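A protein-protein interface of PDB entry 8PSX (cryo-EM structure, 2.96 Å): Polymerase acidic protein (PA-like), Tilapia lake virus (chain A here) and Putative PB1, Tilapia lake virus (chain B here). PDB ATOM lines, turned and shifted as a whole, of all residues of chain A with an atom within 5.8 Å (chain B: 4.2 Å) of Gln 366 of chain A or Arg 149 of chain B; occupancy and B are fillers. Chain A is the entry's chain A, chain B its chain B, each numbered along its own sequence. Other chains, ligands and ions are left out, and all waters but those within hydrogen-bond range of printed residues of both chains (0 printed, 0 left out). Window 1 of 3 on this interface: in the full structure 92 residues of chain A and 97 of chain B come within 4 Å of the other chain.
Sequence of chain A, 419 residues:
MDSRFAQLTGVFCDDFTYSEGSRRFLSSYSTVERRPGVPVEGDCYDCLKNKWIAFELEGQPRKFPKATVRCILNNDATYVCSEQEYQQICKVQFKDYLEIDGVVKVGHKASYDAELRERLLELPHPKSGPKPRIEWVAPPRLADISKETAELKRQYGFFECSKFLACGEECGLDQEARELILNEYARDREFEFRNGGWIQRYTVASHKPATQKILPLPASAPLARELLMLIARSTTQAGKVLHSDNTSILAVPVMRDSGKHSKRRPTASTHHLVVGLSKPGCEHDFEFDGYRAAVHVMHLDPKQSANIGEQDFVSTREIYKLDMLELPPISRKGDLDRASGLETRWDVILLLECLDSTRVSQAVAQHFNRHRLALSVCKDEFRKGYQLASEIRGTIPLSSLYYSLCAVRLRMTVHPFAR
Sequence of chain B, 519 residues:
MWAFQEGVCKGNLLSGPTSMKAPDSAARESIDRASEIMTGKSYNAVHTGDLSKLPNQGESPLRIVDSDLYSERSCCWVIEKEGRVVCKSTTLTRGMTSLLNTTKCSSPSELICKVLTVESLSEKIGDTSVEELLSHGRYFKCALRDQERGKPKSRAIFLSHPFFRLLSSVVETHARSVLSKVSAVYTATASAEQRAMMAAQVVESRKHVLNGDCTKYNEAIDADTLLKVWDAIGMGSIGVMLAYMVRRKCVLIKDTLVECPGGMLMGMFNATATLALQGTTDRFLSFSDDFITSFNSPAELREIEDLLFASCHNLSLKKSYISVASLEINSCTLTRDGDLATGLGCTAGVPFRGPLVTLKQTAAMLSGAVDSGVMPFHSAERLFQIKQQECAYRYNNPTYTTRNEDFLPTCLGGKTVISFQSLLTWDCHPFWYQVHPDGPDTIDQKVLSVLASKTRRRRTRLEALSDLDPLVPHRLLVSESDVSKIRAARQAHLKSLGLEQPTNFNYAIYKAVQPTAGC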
ATOM      1  N   SER A 361      14.919   7.048   0.693  1.00  0.00           N
ATOM      2  CA  SER A 361      14.818   8.468   0.997  1.00  0.00           C
ATOM      3  C   SER A 361      13.597   9.088   0.334  1.00  0.00           C
ATOM      4  O   SER A 361      13.041  10.055   0.855  1.00  0.00           O
ATOM      5  CB  SER A 361      16.088   9.192   0.557  1.00  0.00           C
ATOM      6  OG  SER A 361      16.150   9.302  -0.852  1.00  0.00           O
ATOM      7  N   GLN A 362      13.156   8.541  -0.802  1.00  0.00           N
ATOM      8  CA  GLN A 362      11.945   9.049  -1.438  1.00  0.00           C
ATOM      9  C   GLN A 362      10.716   8.798  -0.573  1.00  0.00           C
ATOM     10  O   GLN A 362       9.861   9.680  -0.422  1.00  0.00           O
ATOM     11  CB  GLN A 362      11.768   8.410  -2.814  1.00  0.00           C
ATOM     12  CG  GLN A 362      12.442   9.174  -3.933  1.00  0.00           C
ATOM     13  CD  GLN A 362      12.733   8.311  -5.141  1.00  0.00           C
ATOM     14  OE1 GLN A 362      12.341   7.147  -5.196  1.00  0.00           O
ATOM     15  NE2 GLN A 362      13.423   8.880  -6.119  1.00  0.00           N
ATOM     16  N   ALA A 363      10.606   7.598   0.002  1.00  0.00           N
ATOM     17  CA  ALA A 363       9.496   7.311   0.904  1.00  0.00           C
ATOM     18  C   ALA A 363       9.553   8.203   2.136  1.00  0.00           C
ATOM     19  O   ALA A 363       8.526   8.739   2.579  1.00  0.00           O
ATOM     20  CB  ALA A 363       9.516   5.838   1.305  1.00  0.00           C
ATOM     21  N   VAL A 364      10.749   8.379   2.702  1.00  0.00           N
ATOM     22  CA  VAL A 364      10.884   9.260   3.859  1.00  0.00           C
ATOM     23  C   VAL A 364      10.472  10.680   3.492  1.00  0.00           C
ATOM     24  O   VAL A 364       9.810  11.371   4.275  1.00  0.00           O
ATOM     25  CB  VAL A 364      12.320   9.210   4.411  1.00  0.00           C
ATOM     26  CG1 VAL A 364      12.454  10.110   5.625  1.00  0.00           C
ATOM     27  CG2 VAL A 364      12.702   7.787   4.771  1.00  0.00           C
ATOM     28  N   ALA A 365      10.858  11.139   2.300  1.00  0.00           N
ATOM     29  CA  ALA A 365      10.522  12.490   1.866  1.00  0.00           C
ATOM     30  C   ALA A 365       9.020  12.664   1.693  1.00  0.00           C
ATOM     31  O   ALA A 365       8.464  13.699   2.074  1.00  0.00           O
ATOM     32  CB  ALA A 365      11.247  12.812   0.561  1.00  0.00           C
ATOM     33  N   GLN A 366       8.348  11.674   1.103  1.00  0.00           N
ATOM     34  CA  GLN A 366       6.898  11.762   0.960  1.00  0.00           C
ATOM     35  C   GLN A 366       6.219  11.819   2.322  1.00  0.00           C
ATOM     36  O   GLN A 366       5.318  12.642   2.552  1.00  0.00           O
ATOM     37  CB  GLN A 366       6.377  10.574   0.154  1.00  0.00           C
ATOM     38  CG  GLN A 366       6.671  10.652  -1.330  1.00  0.00           C
ATOM     39  CD  GLN A 366       6.448   9.331  -2.033  1.00  0.00           C
ATOM     40  OE1 GLN A 366       5.720   8.471  -1.540  1.00  0.00           O
ATOM     41  NE2 GLN A 366       7.071   9.164  -3.191  1.00  0.00           N
ATOM     42  N   HIS A 367       6.648  10.959   3.248  1.00  0.00           N
ATOM     43  CA  HIS A 367       6.042  10.970   4.573  1.00  0.00           C
ATOM     44  C   HIS A 367       6.300  12.293   5.283  1.00  0.00           C
ATOM     45  O   HIS A 367       5.423  12.811   5.979  1.00  0.00           O
ATOM     46  CB  HIS A 367       6.560   9.802   5.409  1.00  0.00           C
ATOM     47  CG  HIS A 367       5.688   9.477   6.579  1.00  0.00           C
ATOM     48  ND1 HIS A 367       4.335   9.248   6.455  1.00  0.00           N
ATOM     49  CD2 HIS A 367       5.970   9.355   7.898  1.00  0.00           C
ATOM     50  CE1 HIS A 367       3.821   8.994   7.645  1.00  0.00           C
ATOM     51  NE2 HIS A 367       4.792   9.052   8.537  1.00  0.00           N
ATOM     52  N   PHE A 368       7.498  12.859   5.118  1.00  0.00           N
ATOM     53  CA  PHE A 368       7.802  14.135   5.756  1.00  0.00           C
ATOM     54  C   PHE A 368       7.012  15.277   5.131  1.00  0.00           C
ATOM     55  O   PHE A 368       6.642  16.227   5.828  1.00  0.00           O
ATOM     56  CB  PHE A 368       9.299  14.421   5.676  1.00  0.00           C
ATOM     57  CG  PHE A 368       9.735  15.594   6.502  1.00  0.00           C
ATOM     58  CD1 PHE A 368       9.423  15.664   7.848  1.00  0.00           C
ATOM     59  CD2 PHE A 368      10.451  16.630   5.934  1.00  0.00           C
ATOM     60  CE1 PHE A 368       9.818  16.744   8.609  1.00  0.00           C
ATOM     61  CE2 PHE A 368      10.851  17.709   6.692  1.00  0.00           C
ATOM     62  CZ  PHE A 368      10.534  17.765   8.030  1.00  0.00           C
ATOM     63  N   ASN A 369       6.757  15.213   3.825  1.00  0.00           N
ATOM     64  CA  ASN A 369       5.876  16.188   3.193  1.00  0.00           C
ATOM     65  C   ASN A 369       4.487  16.132   3.815  1.00  0.00           C
ATOM     66  O   ASN A 369       3.903  17.166   4.170  1.00  0.00           O
ATOM     67  CB  ASN A 369       5.814  15.919   1.690  1.00  0.00           C
ATOM     68  CG  ASN A 369       5.238  17.078   0.912  1.00  0.00           C
ATOM     69  OD1 ASN A 369       5.571  18.235   1.159  1.00  0.00           O
ATOM     70  ND2 ASN A 369       4.371  16.772  -0.044  1.00  0.00           N
ATOM     71  N   ARG A 370       3.950  14.920   3.977  1.00  0.00           N
ATOM     72  CA  ARG A 370       2.663  14.777   4.652  1.00  0.00           C
ATOM     73  C   ARG A 370       2.725  15.331   6.070  1.00  0.00           C
ATOM     74  O   ARG A 370       1.798  16.009   6.524  1.00  0.00           O
ATOM     75  CB  ARG A 370       2.239  13.309   4.684  1.00  0.00           C
ATOM     76  CG  ARG A 370       1.661  12.789   3.386  1.00  0.00           C
ATOM     77  CD  ARG A 370       1.080  11.402   3.578  1.00  0.00           C
ATOM     78  NE  ARG A 370       2.119  10.392   3.726  1.00  0.00           N
ATOM     79  CZ  ARG A 370       2.690   9.744   2.720  1.00  0.00           C
ATOM     80  NH1 ARG A 370       2.347   9.974   1.463  1.00  0.00           N
ATOM     81  NH2 ARG A 370       3.631   8.843   2.981  1.00  0.00           N
ATOM     82  N   HIS A 371       3.814  15.044   6.784  1.00  0.00           N
ATOM     83  CA  HIS A 371       3.974  15.519   8.154  1.00  0.00           C
ATOM     84  C   HIS A 371       3.934  17.040   8.216  1.00  0.00           C
ATOM     85  O   HIS A 371       3.244  17.623   9.060  1.00  0.00           O
ATOM     86  CB  HIS A 371       5.292  14.987   8.720  1.00  0.00           C
ATOM     87  CG  HIS A 371       5.546  15.357  10.148  1.00  0.00           C
ATOM     88  ND1 HIS A 371       6.685  14.972  10.819  1.00  0.00           N
ATOM     89  CD2 HIS A 371       4.812  16.067  11.035  1.00  0.00           C
ATOM     90  CE1 HIS A 371       6.645  15.432  12.056  1.00  0.00           C
ATOM     91  NE2 HIS A 371       5.517  16.101  12.213  1.00  0.00           N
ATOM     92  N   LYS B  10       7.771  16.502  -2.969  1.00  0.00           N
ATOM     93  CA  LYS B  10       7.568  15.059  -2.913  1.00  0.00           C
ATOM     94  C   LYS B  10       8.890  14.301  -2.903  1.00  0.00           C
ATOM     95  O   LYS B  10       8.953  13.180  -2.389  1.00  0.00           O
ATOM     96  CB  LYS B  10       6.718  14.601  -4.097  1.00  0.00           C
ATOM     97  CG  LYS B  10       5.321  14.150  -3.723  1.00  0.00           C
ATOM     98  CD  LYS B  10       4.634  13.466  -4.893  1.00  0.00           C
ATOM     99  CE  LYS B  10       5.006  11.999  -4.980  1.00  0.00           C
ATOM    100  NZ  LYS B  10       4.099  11.248  -5.889  1.00  0.00           N
ATOM    101  N   ASN B  12      10.925  13.950  -5.945  1.00  0.00           N
ATOM    102  CA  ASN B  12      10.909  13.256  -7.224  1.00  0.00           C
ATOM    103  C   ASN B  12      12.163  13.507  -8.054  1.00  0.00           C
ATOM    104  O   ASN B  12      12.213  13.091  -9.215  1.00  0.00           O
ATOM    105  CB  ASN B  12       9.677  13.676  -8.031  1.00  0.00           C
ATOM    106  CG  ASN B  12       8.418  12.958  -7.599  1.00  0.00           C
ATOM    107  OD1 ASN B  12       8.460  12.034  -6.791  1.00  0.00           O
ATOM    108  ND2 ASN B  12       7.284  13.386  -8.137  1.00  0.00           N
ATOM    109  N   LEU B  14      15.261  12.380  -8.011  1.00  0.00           N
ATOM    110  CA  LEU B  14      15.966  11.186  -8.452  1.00  0.00           C
ATOM    111  C   LEU B  14      14.982  10.168  -9.016  1.00  0.00           C
ATOM    112  O   LEU B  14      13.783  10.202  -8.732  1.00  0.00           O
ATOM    113  CB  LEU B  14      16.758  10.561  -7.302  1.00  0.00           C
ATOM    114  CG  LEU B  14      17.869  11.405  -6.671  1.00  0.00           C
ATOM    115  CD1 LEU B  14      18.678  10.559  -5.702  1.00  0.00           C
ATOM    116  CD2 LEU B  14      18.771  12.016  -7.727  1.00  0.00           C
ATOM    117  N   SER B  15      15.507   9.255  -9.828  1.00  0.00           N
ATOM    118  CA  SER B  15      14.676   8.215 -10.410  1.00  0.00           C
ATOM    119  C   SER B  15      14.093   7.327  -9.313  1.00  0.00           C
ATOM    120  O   SER B  15      14.482   7.390  -8.145  1.00  0.00           O
ATOM    121  CB  SER B  15      15.482   7.368 -11.393  1.00  0.00           C
ATOM    122  OG  SER B  15      15.982   8.152 -12.459  1.00  0.00           O
ATOM    123  N   GLY B  16      13.141   6.492  -9.707  1.00  0.00           N
ATOM    124  CA  GLY B  16      12.553   5.536  -8.799  1.00  0.00           C
ATOM    125  C   GLY B  16      13.439   4.327  -8.611  1.00  0.00           C
ATOM    126  O   GLY B  16      14.427   4.111  -9.326  1.00  0.00           O
ATOM    127  N   PRO B  17      13.094   3.510  -7.621  1.00  0.00           N
ATOM    128  CA  PRO B  17      13.896   2.314  -7.348  1.00  0.00           C
ATOM    129  C   PRO B  17      13.814   1.294  -8.473  1.00  0.00           C
ATOM    130  O   PRO B  17      12.802   1.173  -9.166  1.00  0.00           O
ATOM    131  CB  PRO B  17      13.282   1.759  -6.057  1.00  0.00           C
ATOM    132  CG  PRO B  17      11.921   2.341  -5.988  1.00  0.00           C
ATOM    133  CD  PRO B  17      11.982   3.665  -6.670  1.00  0.00           C
ATOM    134  N   GLN B 147      10.372   1.054 -10.267  1.00  0.00           N
ATOM    135  CA  GLN B 147      10.561   2.440 -10.691  1.00  0.00           C
ATOM    136  C   GLN B 147       9.431   3.340 -10.198  1.00  0.00           C
ATOM    137  O   GLN B 147       9.144   4.377 -10.800  1.00  0.00           O
ATOM    138  CB  GLN B 147      10.707   2.549 -12.214  1.00  0.00           C
ATOM    139  CG  GLN B 147      12.149   2.661 -12.692  1.00  0.00           C
ATOM    140  CD  GLN B 147      12.442   1.785 -13.898  1.00  0.00           C
ATOM    141  OE1 GLN B 147      11.542   1.431 -14.660  1.00  0.00           O
ATOM    142  NE2 GLN B 147      13.710   1.433 -14.077  1.00  0.00           N
ATOM    143  N   GLU B 148       8.791   2.957  -9.098  1.00  0.00           N
ATOM    144  CA  GLU B 148       7.793   3.786  -8.436  1.00  0.00           C
ATOM    145  C   GLU B 148       8.445   4.462  -7.238  1.00  0.00           C
ATOM    146  O   GLU B 148       8.879   3.786  -6.300  1.00  0.00           O
ATOM    147  CB  GLU B 148       6.591   2.954  -7.993  1.00  0.00           C
ATOM    148  CG  GLU B 148       5.746   2.424  -9.134  1.00  0.00           C
ATOM    149  CD  GLU B 148       4.333   2.088  -8.701  1.00  0.00           C
ATOM    150  OE1 GLU B 148       3.473   2.993  -8.712  1.00  0.00           O
ATOM    151  OE2 GLU B 148       4.082   0.917  -8.347  1.00  0.00           O
ATOM    152  N   ARG B 149       8.508   5.789  -7.269  1.00  0.00           N
ATOM    153  CA  ARG B 149       9.161   6.526  -6.198  1.00  0.00           C
ATOM    154  C   ARG B 149       8.425   6.316  -4.882  1.00  0.00           C
ATOM    155  O   ARG B 149       7.193   6.266  -4.840  1.00  0.00           O
ATOM    156  CB  ARG B 149       9.221   8.013  -6.545  1.00  0.00           C
ATOM    157  CG  ARG B 149       9.966   8.304  -7.833  1.00  0.00           C
ATOM    158  CD  ARG B 149      10.457   9.734  -7.885  1.00  0.00           C
ATOM    159  NE  ARG B 149      11.183  10.017  -9.116  1.00  0.00           N
ATOM    160  CZ  ARG B 149      10.612  10.227 -10.294  1.00  0.00           C
ATOM    161  NH1 ARG B 149       9.299  10.197 -10.442  1.00  0.00           N
ATOM    162  NH2 ARG B 149      11.379  10.475 -11.351  1.00  0.00           N
ATOM    163  N   GLY B 150       9.191   6.187  -3.802  1.00  0.00           N
ATOM    164  CA  GLY B 150       8.625   5.991  -2.486  1.00  0.00           C
ATOM    165  C   GLY B 150       8.239   4.568  -2.157  1.00  0.00           C
ATOM    166  O   GLY B 150       7.636   4.337  -1.103  1.00  0.00           O
ATOM    167  N   LYS B 151       8.567   3.606  -3.017  1.00  0.00           N
ATOM    168  CA  LYS B 151       8.203   2.202  -2.825  1.00  0.00           C
ATOM    169  C   LYS B 151       9.454   1.348  -2.985  1.00  0.00           C
ATOM    170  O   LYS B 151       9.690   0.768  -4.052  1.00  0.00           O
ATOM    171  CB  LYS B 151       7.117   1.776  -3.813  1.00  0.00           C
ATOM    172  CG  LYS B 151       5.757   2.389  -3.536  1.00  0.00           C
ATOM    173  CD  LYS B 151       4.636   1.554  -4.126  1.00  0.00           C
ATOM    174  CE  LYS B 151       4.336   0.333  -3.274  1.00  0.00           C
ATOM    175  NZ  LYS B 151       3.034   0.449  -2.564  1.00  0.00           N
ATOM    176  N   ALA B 348      10.290  16.523 -11.145  1.00  0.00           N
ATOM    177  CA  ALA B 348      11.199  15.391 -11.198  1.00  0.00           C
ATOM    178  C   ALA B 348      12.440  15.758 -11.996  1.00  0.00           C
ATOM    179  O   ALA B 348      12.411  16.650 -12.847  1.00  0.00           O
ATOM    180  CB  ALA B 348      10.525  14.166 -11.827  1.00  0.00           C
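Hydrophobic or aromatic side chains of chain A that line the printed part of chain B: Ala 363 and Ala 365.
Among the printed residues, merely in contact across the chains: Gln 362 of chain A with Gly 16 of chain B, Gln 362 of chain A with Pro 17 of chain B, Gln 362 of chain A with Arg 149 of chain B, Gln 362 of chain A with Gly 150 of chain B, Ala 363 of chain A with Gly 150 of chain B, Ala 365 of chain A with Lys 10 of chain B, Gln 366 of chain A with Lys 10 of chain B and Gln 366 of chain A with Gly 150 of chain B.
Of chain B, only Lys 10 (3.6 Å), Arg 149 (3.3 Å) and Gly 150 (3.6 Å) come within 4 Å of Gln 366 of chain A. Arg 149 of chain B touches just these residues of chain A: Gln 362 and Gln 366. Of the printed residues of chain A, Gly 150 of chain B touches Gln 362 (3.5 Å), Ala 363 (3.4 Å) and Gln 366 (3.6 Å). Of the printed residues of chain B, Ala 365 of chain A touches Lys 10. Of the printed residues of chain A, Pro 17 of chain B touches Gln 362. Of the printed residues of chain A, Leu 14 of chain B touches Gln 362. Lys 151 of chain B touches none of the printed residues of chain A. Arg 370 of chain A touches none of the printed residues of chain B. The nearest residue of chain A that does not touch Arg 149 of chain B is Ala 363 of chain A (5.5 Å). The nearest printed residue of chain A that does not touch Ser 15 of chain B is Ser 361 of chain A (7.7 Å).
The backbone carbonyl oxygen (O) of Arg 149 of chain B sits at hydrogen-bond distance from the side-chain amide nitrogen (NE2) of Gln 366 of chain A (3.3 Å). O of Leu 14 of chain B sits at hydrogen-bond distance from NE2 of Gln 362 of chain A (3.0 Å). The side-chain amide nitrogen (NE2) of Gln 362 of chain A is in hydrogen-bond range of the backbone carbonyl oxygen (O) of Ser 15 of chain B (2.7 Å).
The backbone carbonyl oxygen (O) of Asn 12 of chain B lies within hydrogen-bond range of the guanidinium group (NE) of Arg 149 of chain B. O of Leu 14 of chain B sits at hydrogen-bond distance from NE of Arg 149 of chain B (2.6 Å). The backbone carbonyl oxygen (O) of Pro 17 of chain B is in hydrogen-bond range of the backbone NH (N) of Gln 147 of chain B, at 2.7 Å.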
